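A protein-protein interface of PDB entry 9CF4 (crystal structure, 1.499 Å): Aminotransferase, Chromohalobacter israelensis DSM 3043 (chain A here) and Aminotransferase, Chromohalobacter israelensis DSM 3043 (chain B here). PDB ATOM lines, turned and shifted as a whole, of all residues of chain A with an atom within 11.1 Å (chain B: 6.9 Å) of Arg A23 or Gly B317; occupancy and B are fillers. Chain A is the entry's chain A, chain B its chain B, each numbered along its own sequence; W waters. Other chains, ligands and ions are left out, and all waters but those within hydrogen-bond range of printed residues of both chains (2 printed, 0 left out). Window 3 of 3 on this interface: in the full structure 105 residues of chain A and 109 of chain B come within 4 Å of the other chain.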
ATOM      1  N   ASP A  11     -35.126 -31.172  -1.480  1.00  0.00           N
ATOM      2  CA  ASP A  11     -33.732 -31.230  -1.043  1.00  0.00           C
ATOM      3  C   ASP A  11     -32.851 -30.326  -1.897  1.00  0.00           C
ATOM      4  O   ASP A  11     -31.895 -29.717  -1.397  1.00  0.00           O
ATOM      5  CB  ASP A  11     -33.276 -32.688  -1.125  1.00  0.00           C
ATOM      6  CG  ASP A  11     -31.948 -32.932  -0.440  1.00  0.00           C
ATOM      7  OD1 ASP A  11     -31.755 -32.457   0.694  1.00  0.00           O
ATOM      8  OD2 ASP A  11     -31.106 -33.637  -1.031  1.00  0.00           O
ATOM      9  N   ARG A  12     -33.145 -30.229  -3.189  1.00  0.00           N
ATOM     10  CA  ARG A  12     -32.320 -29.382  -4.042  1.00  0.00           C
ATOM     11  C   ARG A  12     -32.283 -27.940  -3.556  1.00  0.00           C
ATOM     12  O   ARG A  12     -31.301 -27.218  -3.805  1.00  0.00           O
ATOM     13  CB  ARG A  12     -32.866 -29.379  -5.470  1.00  0.00           C
ATOM     14  CG  ARG A  12     -32.852 -30.703  -6.191  1.00  0.00           C
ATOM     15  CD  ARG A  12     -33.370 -30.522  -7.625  1.00  0.00           C
ATOM     16  NE  ARG A  12     -33.641 -31.796  -8.260  1.00  0.00           N
ATOM     17  CZ  ARG A  12     -32.707 -32.569  -8.803  1.00  0.00           C
ATOM     18  NH1 ARG A  12     -31.451 -32.161  -8.797  1.00  0.00           N
ATOM     19  NH2 ARG A  12     -33.037 -33.731  -9.356  1.00  0.00           N
ATOM     20  N   LYS A  13     -33.366 -27.480  -2.926  1.00  0.00           N
ATOM     21  CA  LYS A  13     -33.447 -26.100  -2.486  1.00  0.00           C
ATOM     22  C   LYS A  13     -32.721 -25.827  -1.176  1.00  0.00           C
ATOM     23  O   LYS A  13     -32.511 -24.652  -0.843  1.00  0.00           O
ATOM     24  CB  LYS A  13     -34.900 -25.712  -2.299  1.00  0.00           C
ATOM     25  CG  LYS A  13     -35.666 -25.723  -3.578  1.00  0.00           C
ATOM     26  CD  LYS A  13     -37.087 -25.334  -3.333  1.00  0.00           C
ATOM     27  CE  LYS A  13     -37.838 -25.403  -4.632  1.00  0.00           C
ATOM     28  NZ  LYS A  13     -37.307 -24.448  -5.601  1.00  0.00           N
ATOM     29  N   VAL A  14     -32.326 -26.856  -0.429  1.00  0.00           N
ATOM     30  CA  VAL A  14     -31.935 -26.649   0.962  1.00  0.00           C
ATOM     31  C   VAL A  14     -30.641 -27.325   1.374  1.00  0.00           C
ATOM     32  O   VAL A  14     -30.067 -26.903   2.390  1.00  0.00           O
ATOM     33  CB  VAL A  14     -33.072 -27.033   1.944  1.00  0.00           C
ATOM     34  CG1 VAL A  14     -34.242 -26.077   1.768  1.00  0.00           C
ATOM     35  CG2 VAL A  14     -33.525 -28.498   1.756  1.00  0.00           C
ATOM     36  N   THR A  15     -30.145 -28.377   0.713  1.00  0.00           N
ATOM     37  CA  THR A  15     -29.023 -29.144   1.244  1.00  0.00           C
ATOM     38  C   THR A  15     -27.804 -29.088   0.333  1.00  0.00           C
ATOM     39  O   THR A  15     -27.907 -29.320  -0.877  1.00  0.00           O
ATOM     40  CB  THR A  15     -29.422 -30.614   1.491  1.00  0.00           C
ATOM     41  OG1 THR A  15     -30.560 -30.676   2.361  1.00  0.00           O
ATOM     42  CG2 THR A  15     -28.244 -31.375   2.104  1.00  0.00           C
ATOM     43  N   PHE A  16     -26.644 -28.801   0.933  1.00  0.00           N
ATOM     44  CA  PHE A  16     -25.311 -28.947   0.320  1.00  0.00           C
ATOM     45  C   PHE A  16     -24.858 -30.356   0.671  1.00  0.00           C
ATOM     46  O   PHE A  16     -24.625 -30.665   1.833  1.00  0.00           O
ATOM     47  CB  PHE A  16     -24.418 -27.854   0.911  1.00  0.00           C
ATOM     48  CG  PHE A  16     -22.914 -27.925   0.634  1.00  0.00           C
ATOM     49  CD1 PHE A  16     -22.238 -29.047   0.187  1.00  0.00           C
ATOM     50  CD2 PHE A  16     -22.166 -26.797   0.931  1.00  0.00           C
ATOM     51  CE1 PHE A  16     -20.850 -29.020   0.054  1.00  0.00           C
ATOM     52  CE2 PHE A  16     -20.792 -26.760   0.769  1.00  0.00           C
ATOM     53  CZ  PHE A  16     -20.143 -27.869   0.342  1.00  0.00           C
ATOM     54  N   HIS A  17     -24.761 -31.208  -0.336  1.00  0.00           N
ATOM     55  CA  HIS A  17     -24.327 -32.580  -0.150  1.00  0.00           C
ATOM     56  C   HIS A  17     -22.847 -32.767  -0.440  1.00  0.00           C
ATOM     57  O   HIS A  17     -22.280 -32.149  -1.348  1.00  0.00           O
ATOM     58  CB  HIS A  17     -25.094 -33.521  -1.091  1.00  0.00           C
ATOM     59  CG  HIS A  17     -26.496 -33.780  -0.678  1.00  0.00           C
ATOM     60  ND1 HIS A  17     -26.810 -34.697   0.295  1.00  0.00           N
ATOM     61  CD2 HIS A  17     -27.671 -33.249  -1.099  1.00  0.00           C
ATOM     62  CE1 HIS A  17     -28.121 -34.722   0.464  1.00  0.00           C
ATOM     63  NE2 HIS A  17     -28.667 -33.854  -0.375  1.00  0.00           N
ATOM     64  N   ALA A  18     -22.242 -33.663   0.335  1.00  0.00           N
ATOM     65  CA  ALA A  18     -20.889 -34.119   0.057  1.00  0.00           C
ATOM     66  C   ALA A  18     -20.732 -34.594  -1.380  1.00  0.00           C
ATOM     67  O   ALA A  18     -21.630 -35.215  -1.961  1.00  0.00           O
ATOM     68  CB  ALA A  18     -20.550 -35.275   1.008  1.00  0.00           C
ATOM     69  N   SER A  19     -19.561 -34.315  -1.947  1.00  0.00           N
ATOM     70  CA  SER A  19     -19.169 -34.824  -3.261  1.00  0.00           C
ATOM     71  C   SER A  19     -20.302 -34.728  -4.271  1.00  0.00           C
ATOM     72  O   SER A  19     -20.643 -35.690  -4.962  1.00  0.00           O
ATOM     73  CB  SER A  19     -18.668 -36.264  -3.155  1.00  0.00           C
ATOM     74  OG  SER A  19     -17.544 -36.333  -2.315  1.00  0.00           O
ATOM     75  N   THR A  20     -20.886 -33.546  -4.359  1.00  0.00           N
ATOM     76  CA  THR A  20     -21.995 -33.297  -5.275  1.00  0.00           C
ATOM     77  C   THR A  20     -21.688 -32.116  -6.180  1.00  0.00           C
ATOM     78  O   THR A  20     -20.987 -31.175  -5.798  1.00  0.00           O
ATOM     79  CB  THR A  20     -23.291 -33.074  -4.461  1.00  0.00           C
ATOM     80  OG1 THR A  20     -23.622 -34.285  -3.754  1.00  0.00           O
ATOM     81  CG2 THR A  20     -24.469 -32.666  -5.317  1.00  0.00           C
ATOM     82  N   HIS A  21     -22.181 -32.212  -7.413  1.00  0.00           N
ATOM     83  CA  HIS A  21     -22.129 -31.099  -8.344  1.00  0.00           C
ATOM     84  C   HIS A  21     -23.150 -30.072  -7.862  1.00  0.00           C
ATOM     85  O   HIS A  21     -24.345 -30.179  -8.173  1.00  0.00           O
ATOM     86  CB  HIS A  21     -22.471 -31.563  -9.744  1.00  0.00           C
ATOM     87  CG  HIS A  21     -22.074 -30.580 -10.791  1.00  0.00           C
ATOM     88  ND1 HIS A  21     -22.561 -29.291 -10.814  1.00  0.00           N
ATOM     89  CD2 HIS A  21     -21.229 -30.686 -11.843  1.00  0.00           C
ATOM     90  CE1 HIS A  21     -22.042 -28.654 -11.851  1.00  0.00           C
ATOM     91  NE2 HIS A  21     -21.218 -29.472 -12.478  1.00  0.00           N
ATOM     92  N   LEU A  22     -22.699 -29.126  -7.048  1.00  0.00           N
ATOM     93  CA  LEU A  22     -23.635 -28.285  -6.303  1.00  0.00           C
ATOM     94  C   LEU A  22     -24.540 -27.494  -7.238  1.00  0.00           C
ATOM     95  O   LEU A  22     -25.739 -27.382  -6.988  1.00  0.00           O
ATOM     96  CB  LEU A  22     -22.864 -27.357  -5.361  1.00  0.00           C
ATOM     97  CG  LEU A  22     -22.043 -28.092  -4.292  1.00  0.00           C
ATOM     98  CD1 LEU A  22     -21.348 -27.079  -3.379  1.00  0.00           C
ATOM     99  CD2 LEU A  22     -22.892 -29.072  -3.471  1.00  0.00           C
ATOM    100  N   ARG A  23     -23.989 -26.937  -8.319  1.00  0.00           N
ATOM    101  CA  ARG A  23     -24.816 -26.173  -9.243  1.00  0.00           C
ATOM    102  C   ARG A  23     -25.847 -27.072  -9.912  1.00  0.00           C
ATOM    103  O   ARG A  23     -27.042 -26.745  -9.949  1.00  0.00           O
ATOM    104  CB  ARG A  23     -23.951 -25.481 -10.297  1.00  0.00           C
ATOM    105  CG  ARG A  23     -24.762 -24.567 -11.220  1.00  0.00           C
ATOM    106  CD  ARG A  23     -24.017 -24.236 -12.506  1.00  0.00           C
ATOM    107  NE  ARG A  23     -23.812 -25.437 -13.309  1.00  0.00           N
ATOM    108  CZ  ARG A  23     -23.106 -25.474 -14.432  1.00  0.00           C
ATOM    109  NH1 ARG A  23     -22.538 -24.365 -14.891  1.00  0.00           N
ATOM    110  NH2 ARG A  23     -22.964 -26.619 -15.087  1.00  0.00           N
ATOM    111  N   ASP A  24     -25.397 -28.196 -10.490  1.00  0.00           N
ATOM    112  CA  ASP A  24     -26.340 -29.032 -11.231  1.00  0.00           C
ATOM    113  C   ASP A  24     -27.406 -29.629 -10.310  1.00  0.00           C
ATOM    114  O   ASP A  24     -28.564 -29.779 -10.723  1.00  0.00           O
ATOM    115  CB  ASP A  24     -25.629 -30.136 -12.010  1.00  0.00           C
ATOM    116  CG  ASP A  24     -24.878 -29.622 -13.229  1.00  0.00           C
ATOM    117  OD1 ASP A  24     -24.980 -28.407 -13.557  1.00  0.00           O
ATOM    118  OD2 ASP A  24     -24.163 -30.444 -13.853  1.00  0.00           O
ATOM    119  N   PHE A  25     -27.055 -29.960  -9.069  1.00  0.00           N
ATOM    120  CA  PHE A  25     -28.074 -30.503  -8.169  1.00  0.00           C
ATOM    121  C   PHE A  25     -29.096 -29.438  -7.770  1.00  0.00           C
ATOM    122  O   PHE A  25     -30.305 -29.683  -7.803  1.00  0.00           O
ATOM    123  CB  PHE A  25     -27.427 -31.141  -6.945  1.00  0.00           C
ATOM    124  CG  PHE A  25     -28.404 -31.861  -6.068  1.00  0.00           C
ATOM    125  CD1 PHE A  25     -28.921 -33.086  -6.454  1.00  0.00           C
ATOM    126  CD2 PHE A  25     -28.824 -31.306  -4.878  1.00  0.00           C
ATOM    127  CE1 PHE A  25     -29.845 -33.742  -5.646  1.00  0.00           C
ATOM    128  CE2 PHE A  25     -29.724 -31.963  -4.076  1.00  0.00           C
ATOM    129  CZ  PHE A  25     -30.234 -33.171  -4.463  1.00  0.00           C
ATOM    130  N   ALA A  26     -28.638 -28.239  -7.409  1.00  0.00           N
ATOM    131  CA  ALA A  26     -29.572 -27.180  -7.033  1.00  0.00           C
ATOM    132  C   ALA A  26     -30.509 -26.801  -8.175  1.00  0.00           C
ATOM    133  O   ALA A  26     -31.672 -26.427  -7.938  1.00  0.00           O
ATOM    134  CB  ALA A  26     -28.803 -25.951  -6.557  1.00  0.00           C
ATOM    135  N   HIS A  27     -30.040 -26.913  -9.411  1.00  0.00           N
ATOM    136  CA  HIS A  27     -30.796 -26.444 -10.569  1.00  0.00           C
ATOM    137  C   HIS A  27     -31.542 -27.558 -11.300  1.00  0.00           C
ATOM    138  O   HIS A  27     -32.138 -27.305 -12.350  1.00  0.00           O
ATOM    139  CB  HIS A  27     -29.888 -25.678 -11.531  1.00  0.00           C
ATOM    140  CG  HIS A  27     -29.474 -24.341 -11.012  1.00  0.00           C
ATOM    141  ND1 HIS A  27     -30.181 -23.187 -11.271  1.00  0.00           N
ATOM    142  CD2 HIS A  27     -28.442 -23.979 -10.220  1.00  0.00           C
ATOM    143  CE1 HIS A  27     -29.585 -22.168 -10.677  1.00  0.00           C
ATOM    144  NE2 HIS A  27     -28.522 -22.623 -10.040  1.00  0.00           N
ATOM    145  N   GLY A  28     -31.556 -28.772 -10.755  1.00  0.00           N
ATOM    146  CA  GLY A  28     -32.398 -29.827 -11.277  1.00  0.00           C
ATOM    147  C   GLY A  28     -31.784 -30.705 -12.346  1.00  0.00           C
ATOM    148  O   GLY A  28     -32.487 -31.576 -12.886  1.00  0.00           O
ATOM    149  N   GLU A  29     -30.499 -30.524 -12.661  1.00  0.00           N
ATOM    150  CA  GLU A  29     -29.874 -31.301 -13.720  1.00  0.00           C
ATOM    151  C   GLU A  29     -29.185 -32.565 -13.222  1.00  0.00           C
ATOM    152  O   GLU A  29     -29.097 -33.543 -13.972  1.00  0.00           O
ATOM    153  CB  GLU A  29     -28.853 -30.463 -14.492  1.00  0.00           C
ATOM    154  CG  GLU A  29     -29.423 -29.664 -15.653  1.00  0.00           C
ATOM    155  CD  GLU A  29     -29.799 -28.271 -15.251  1.00  0.00           C
ATOM    156  OE1 GLU A  29     -30.372 -28.121 -14.150  1.00  0.00           O
ATOM    157  OE2 GLU A  29     -29.511 -27.326 -16.023  1.00  0.00           O
ATOM    158  N   ALA A  30     -28.719 -32.589 -12.019  1.00  0.00           N
ATOM    159  CA  ALA A  30     -28.068 -33.789 -11.511  1.00  0.00           C
ATOM    160  C   ALA A  30     -29.062 -34.620 -10.719  1.00  0.00           C
ATOM    161  O   ALA A  30     -29.961 -34.070 -10.075  1.00  0.00           O
ATOM    162  CB  ALA A  30     -26.915 -33.425 -10.575  1.00  0.00           C
ATOM    163  N   PRO A  31     -28.938 -35.944 -10.730  1.00  0.00           N
ATOM    164  CA  PRO A  31     -29.939 -36.783 -10.065  1.00  0.00           C
ATOM    165  C   PRO A  31     -29.757 -36.818  -8.553  1.00  0.00           C
ATOM    166  O   PRO A  31     -28.666 -36.622  -8.007  1.00  0.00           O
ATOM    167  CB  PRO A  31     -29.671 -38.170 -10.655  1.00  0.00           C
ATOM    168  CG  PRO A  31     -28.217 -38.169 -10.959  1.00  0.00           C
ATOM    169  CD  PRO A  31     -27.927 -36.747 -11.448  1.00  0.00           C
ATOM    170  N   HIS A 171      -8.157 -26.253  -5.229  1.00  0.00           N
ATOM    171  CA  HIS A 171      -9.064 -25.157  -4.913  1.00  0.00           C
ATOM    172  C   HIS A 171      -9.150 -24.908  -3.405  1.00  0.00           C
ATOM    173  O   HIS A 171      -9.795 -23.943  -2.996  1.00  0.00           O
ATOM    174  CB  HIS A 171     -10.459 -25.393  -5.499  1.00  0.00           C
ATOM    175  CG  HIS A 171     -10.435 -25.863  -6.916  1.00  0.00           C
ATOM    176  ND1 HIS A 171      -9.895 -25.119  -7.944  1.00  0.00           N
ATOM    177  CD2 HIS A 171     -10.841 -27.031  -7.468  1.00  0.00           C
ATOM    178  CE1 HIS A 171      -9.996 -25.801  -9.076  1.00  0.00           C
ATOM    179  NE2 HIS A 171     -10.554 -26.970  -8.809  1.00  0.00           N
ATOM    180  N   TYR B 132     -12.093 -21.989  -1.237  1.00  0.00           N
ATOM    181  CA  TYR B 132     -12.702 -22.317  -2.521  1.00  0.00           C
ATOM    182  C   TYR B 132     -13.327 -21.074  -3.141  1.00  0.00           C
ATOM    183  O   TYR B 132     -13.105 -20.777  -4.318  1.00  0.00           O
ATOM    184  CB  TYR B 132     -13.752 -23.417  -2.283  1.00  0.00           C
ATOM    185  CG  TYR B 132     -14.372 -24.035  -3.521  1.00  0.00           C
ATOM    186  CD1 TYR B 132     -15.519 -23.487  -4.083  1.00  0.00           C
ATOM    187  CD2 TYR B 132     -13.838 -25.162  -4.112  1.00  0.00           C
ATOM    188  CE1 TYR B 132     -16.110 -24.052  -5.212  1.00  0.00           C
ATOM    189  CE2 TYR B 132     -14.403 -25.723  -5.243  1.00  0.00           C
ATOM    190  CZ  TYR B 132     -15.551 -25.165  -5.796  1.00  0.00           C
ATOM    191  OH  TYR B 132     -16.122 -25.708  -6.928  1.00  0.00           O
ATOM    192  N   TRP B 309     -23.052 -19.085  -1.671  1.00  0.00           N
ATOM    193  CA  TRP B 309     -23.613 -20.191  -2.433  1.00  0.00           C
ATOM    194  C   TRP B 309     -23.480 -19.947  -3.933  1.00  0.00           C
ATOM    195  O   TRP B 309     -23.219 -20.878  -4.704  1.00  0.00           O
ATOM    196  CB  TRP B 309     -25.085 -20.427  -2.063  1.00  0.00           C
ATOM    197  CG  TRP B 309     -25.612 -21.604  -2.791  1.00  0.00           C
ATOM    198  CD1 TRP B 309     -26.477 -21.598  -3.835  1.00  0.00           C
ATOM    199  CD2 TRP B 309     -25.259 -22.969  -2.565  1.00  0.00           C
ATOM    200  NE1 TRP B 309     -26.709 -22.893  -4.270  1.00  0.00           N
ATOM    201  CE2 TRP B 309     -25.966 -23.747  -3.500  1.00  0.00           C
ATOM    202  CE3 TRP B 309     -24.415 -23.615  -1.658  1.00  0.00           C
ATOM    203  CZ2 TRP B 309     -25.858 -25.140  -3.543  1.00  0.00           C
ATOM    204  CZ3 TRP B 309     -24.301 -24.983  -1.715  1.00  0.00           C
ATOM    205  CH2 TRP B 309     -25.030 -25.732  -2.642  1.00  0.00           C
ATOM    206  N   VAL B 311     -21.139 -18.532  -5.559  1.00  0.00           N
ATOM    207  CA  VAL B 311     -19.787 -18.867  -6.004  1.00  0.00           C
ATOM    208  C   VAL B 311     -19.538 -20.371  -5.911  1.00  0.00           C
ATOM    209  O   VAL B 311     -18.820 -20.924  -6.747  1.00  0.00           O
ATOM    210  CB  VAL B 311     -18.767 -18.036  -5.216  1.00  0.00           C
ATOM    211  CG1 VAL B 311     -17.318 -18.381  -5.585  1.00  0.00           C
ATOM    212  CG2 VAL B 311     -19.009 -16.547  -5.519  1.00  0.00           C
ATOM    213  N   LEU B 312     -20.139 -21.063  -4.929  1.00  0.00           N
ATOM    214  CA  LEU B 312     -20.068 -22.524  -4.929  1.00  0.00           C
ATOM    215  C   LEU B 312     -20.708 -23.099  -6.187  1.00  0.00           C
ATOM    216  O   LEU B 312     -20.221 -24.085  -6.742  1.00  0.00           O
ATOM    217  CB  LEU B 312     -20.695 -23.104  -3.658  1.00  0.00           C
ATOM    218  CG  LEU B 312     -20.014 -22.739  -2.340  1.00  0.00           C
ATOM    219  CD1 LEU B 312     -20.723 -23.346  -1.108  1.00  0.00           C
ATOM    220  CD2 LEU B 312     -18.544 -23.141  -2.306  1.00  0.00           C
ATOM    221  N   GLU B 313     -21.820 -22.509  -6.645  1.00  0.00           N
ATOM    222  CA  GLU B 313     -22.407 -22.943  -7.913  1.00  0.00           C
ATOM    223  C   GLU B 313     -21.466 -22.645  -9.079  1.00  0.00           C
ATOM    224  O   GLU B 313     -21.234 -23.497  -9.940  1.00  0.00           O
ATOM    225  CB  GLU B 313     -23.766 -22.289  -8.137  1.00  0.00           C
ATOM    226  CG  GLU B 313     -24.866 -22.807  -7.188  1.00  0.00           C
ATOM    227  CD  GLU B 313     -26.280 -22.422  -7.613  1.00  0.00           C
ATOM    228  OE1 GLU B 313     -26.443 -21.545  -8.492  1.00  0.00           O
ATOM    229  OE2 GLU B 313     -27.245 -22.988  -7.048  1.00  0.00           O
ATOM    230  N   GLN B 314     -20.890 -21.449  -9.113  1.00  0.00           N
ATOM    231  CA  GLN B 314     -20.016 -21.128 -10.234  1.00  0.00           C
ATOM    232  C   GLN B 314     -18.833 -22.087 -10.274  1.00  0.00           C
ATOM    233  O   GLN B 314     -18.455 -22.585 -11.337  1.00  0.00           O
ATOM    234  CB  GLN B 314     -19.524 -19.684 -10.148  1.00  0.00           C
ATOM    235  CG  GLN B 314     -18.727 -19.308 -11.371  1.00  0.00           C
ATOM    236  CD  GLN B 314     -18.214 -17.885 -11.373  1.00  0.00           C
ATOM    237  OE1 GLN B 314     -17.899 -17.314 -10.335  1.00  0.00           O
ATOM    238  NE2 GLN B 314     -18.132 -17.295 -12.577  1.00  0.00           N
ATOM    239  N   GLY B 315     -18.263 -22.384  -9.110  1.00  0.00           N
ATOM    240  CA  GLY B 315     -17.081 -23.230  -9.062  1.00  0.00           C
ATOM    241  C   GLY B 315     -17.369 -24.661  -9.455  1.00  0.00           C
ATOM    242  O   GLY B 315     -16.592 -25.278 -10.194  1.00  0.00           O
ATOM    243  N   THR B 316     -18.484 -25.215  -8.974  1.00  0.00           N
ATOM    244  CA  THR B 316     -18.836 -26.581  -9.364  1.00  0.00           C
ATOM    245  C   THR B 316     -19.220 -26.644 -10.829  1.00  0.00           C
ATOM    246  O   THR B 316     -18.927 -27.640 -11.498  1.00  0.00           O
ATOM    247  CB  THR B 316     -19.890 -27.189  -8.432  1.00  0.00           C
ATOM    248  OG1 THR B 316     -21.077 -26.392  -8.383  1.00  0.00           O
ATOM    249  CG2 THR B 316     -19.312 -27.363  -7.028  1.00  0.00           C
ATOM    250  N   GLY B 317     -19.801 -25.573 -11.360  1.00  0.00           N
ATOM    251  CA  GLY B 317     -20.048 -25.523 -12.792  1.00  0.00           C
ATOM    252  C   GLY B 317     -18.764 -25.617 -13.586  1.00  0.00           C
ATOM    253  O   GLY B 317     -18.724 -26.235 -14.652  1.00  0.00           O
ATOM    254  N   GLU B 318     -17.685 -25.017 -13.065  1.00  0.00           N
ATOM    255  CA  GLU B 318     -16.405 -25.032 -13.764  1.00  0.00           C
ATOM    256  C   GLU B 318     -15.620 -26.316 -13.499  1.00  0.00           C
ATOM    257  O   GLU B 318     -14.991 -26.860 -14.420  1.00  0.00           O
ATOM    258  CB  GLU B 318     -15.596 -23.794 -13.357  1.00  0.00           C
ATOM    259  CG  GLU B 318     -14.291 -23.644 -14.090  1.00  0.00           C
ATOM    260  CD  GLU B 318     -13.631 -22.297 -13.845  1.00  0.00           C
ATOM    261  OE1 GLU B 318     -14.186 -21.464 -13.083  1.00  0.00           O
ATOM    262  OE2 GLU B 318     -12.547 -22.076 -14.434  1.00  0.00           O
ATOM    263  N   PHE B 319     -15.649 -26.823 -12.271  1.00  0.00           N
ATOM    264  CA  PHE B 319     -14.707 -27.846 -11.842  1.00  0.00           C
ATOM    265  C   PHE B 319     -15.348 -29.178 -11.471  1.00  0.00           C
ATOM    266  O   PHE B 319     -14.611 -30.156 -11.258  1.00  0.00           O
ATOM    267  CB  PHE B 319     -13.890 -27.330 -10.643  1.00  0.00           C
ATOM    268  CG  PHE B 319     -13.085 -26.106 -10.952  1.00  0.00           C
ATOM    269  CD1 PHE B 319     -12.134 -26.126 -11.961  1.00  0.00           C
ATOM    270  CD2 PHE B 319     -13.256 -24.941 -10.238  1.00  0.00           C
ATOM    271  CE1 PHE B 319     -11.392 -25.004 -12.249  1.00  0.00           C
ATOM    272  CE2 PHE B 319     -12.510 -23.813 -10.532  1.00  0.00           C
ATOM    273  CZ  PHE B 319     -11.581 -23.848 -11.531  1.00  0.00           C
ATOM    274  N   GLY B 320     -16.674 -29.244 -11.382  1.00  0.00           N
ATOM    275  CA  GLY B 320     -17.365 -30.478 -11.057  1.00  0.00           C
ATOM    276  C   GLY B 320     -17.653 -30.644  -9.576  1.00  0.00           C
ATOM    277  O   GLY B 320     -17.564 -29.701  -8.776  1.00  0.00           O
ATOM    278  N   PRO B 321     -18.040 -31.846  -9.190  1.00  0.00           N
ATOM    279  CA  PRO B 321     -18.458 -32.073  -7.802  1.00  0.00           C
ATOM    280  C   PRO B 321     -17.424 -31.613  -6.784  1.00  0.00           C
ATOM    281  O   PRO B 321     -16.212 -31.785  -6.961  1.00  0.00           O
ATOM    282  CB  PRO B 321     -18.661 -33.589  -7.746  1.00  0.00           C
ATOM    283  CG  PRO B 321     -18.995 -33.980  -9.168  1.00  0.00           C
ATOM    284  CD  PRO B 321     -18.165 -33.058 -10.026  1.00  0.00           C
HETATM  285  O   HOH W   1     -19.724 -28.709 -14.900  1.00  0.00           O
HETATM  286  O   HOH W   2     -29.687 -22.030  -6.844  1.00  0.00           O
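Among the printed residues, pairs that only touch across the chains: Thr A20 with Pro B321 (3.3 Å), Arg A23 with Glu B313 (3.4 Å), Ala A26 with Glu B313 (3.4 Å), His A171 with Phe B319 (3.4 Å), Arg A23 with Gly B317 (3.5 Å), His A21 with Pro B321 (3.7 Å), His A21 with Gly B317 (3.8 Å), Leu A22 with Trp B309 (3.8 Å), Phe A16 with Trp B309 (3.9 Å), Phe A16 with Leu B312 (3.9 Å) and His A21 with Gly B320 (3.9 Å).
Of the 22 printed residues of chain A, 8 touch a printed residue of chain B. Hydrophobic or aromatic side chains of chain A that line the printed part of chain B: Phe A16, His A21, Leu A22, Ala A26, His A27 and His A171. Among the printed residues, no Asp or Glu carboxylate lies within 4 Å of a Lys or Arg side-chain nitrogen of the other chain.
NH2 of Arg A23 is in salt-bridge range of OD1 of Asp A24 (3.1 Å). NE1 of Trp B309 lies within hydrogen-bond range of OE2 of Glu B313. O of His A27 lies close to OE1 of Glu A29 (2.7 Å). OH of Tyr B132 lies within hydrogen-bond range of N of Thr B316 (3.2 Å). The side-chain hydroxyl (OG1) of Thr B316 sits at hydrogen-bond distance from the backbone carbonyl oxygen (O) of Glu B313 (3.3 Å). OH of Tyr B132 sits close to O of Gly B315, 3.3 Å away.
Printed residues of chain B within 4 Å of His A21: Thr B316, Gly B317, Gly B320 and Pro B321. Printed residues of chain B within 4 Å of Leu A22: Trp B309 (3.8 Å) and Thr B316 (3.4 Å). Arg A23 touches three residues of chain B. Glu B313 touches three residues of chain A. Thr B316 touches just these residues of chain A: His A21 (3.1 Å), Leu A22 (3.4 Å) and Arg A23 (3.0 Å). Gly B317 touches two residues of chain A. Of chain A, only His A21 (3.9 Å) comes within 4 Å of Gly B320. The nearest residue of chain B that does not touch Arg A23 is Leu B312 (5.0 Å). The nearest residue of chain A that does not touch Gly B317 is Asp A24 (5.8 Å). The nearest printed residue of chain A that does not touch Trp B309 is Ala A26 (4.3 Å).
OG1 of Thr B316 is in hydrogen-bond range of N of Arg A23, 3.0 Å away. A ring nitrogen (NE2) of His A21 is in hydrogen-bond range of the backbone carbonyl oxygen (O) of Thr B316. A ring nitrogen (NE2) of His A27 lies within hydrogen-bond range of the side-chain carboxylate (OE1) of Glu B313, 2.8 Å away. OG1 of Thr B316 is in hydrogen-bond range of N of Leu A22. The backbone NH (N) of Tyr B132 lies close to the backbone carbonyl oxygen (O) of His A171.
Water W2 lies within hydrogen-bond range of OE2 of Glu B313 and NE2 of His A27. Water W1 lies within hydrogen-bond range of the backbone carbonyl oxygen of Gly B317 and a ring nitrogen (NE2) of His A21.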
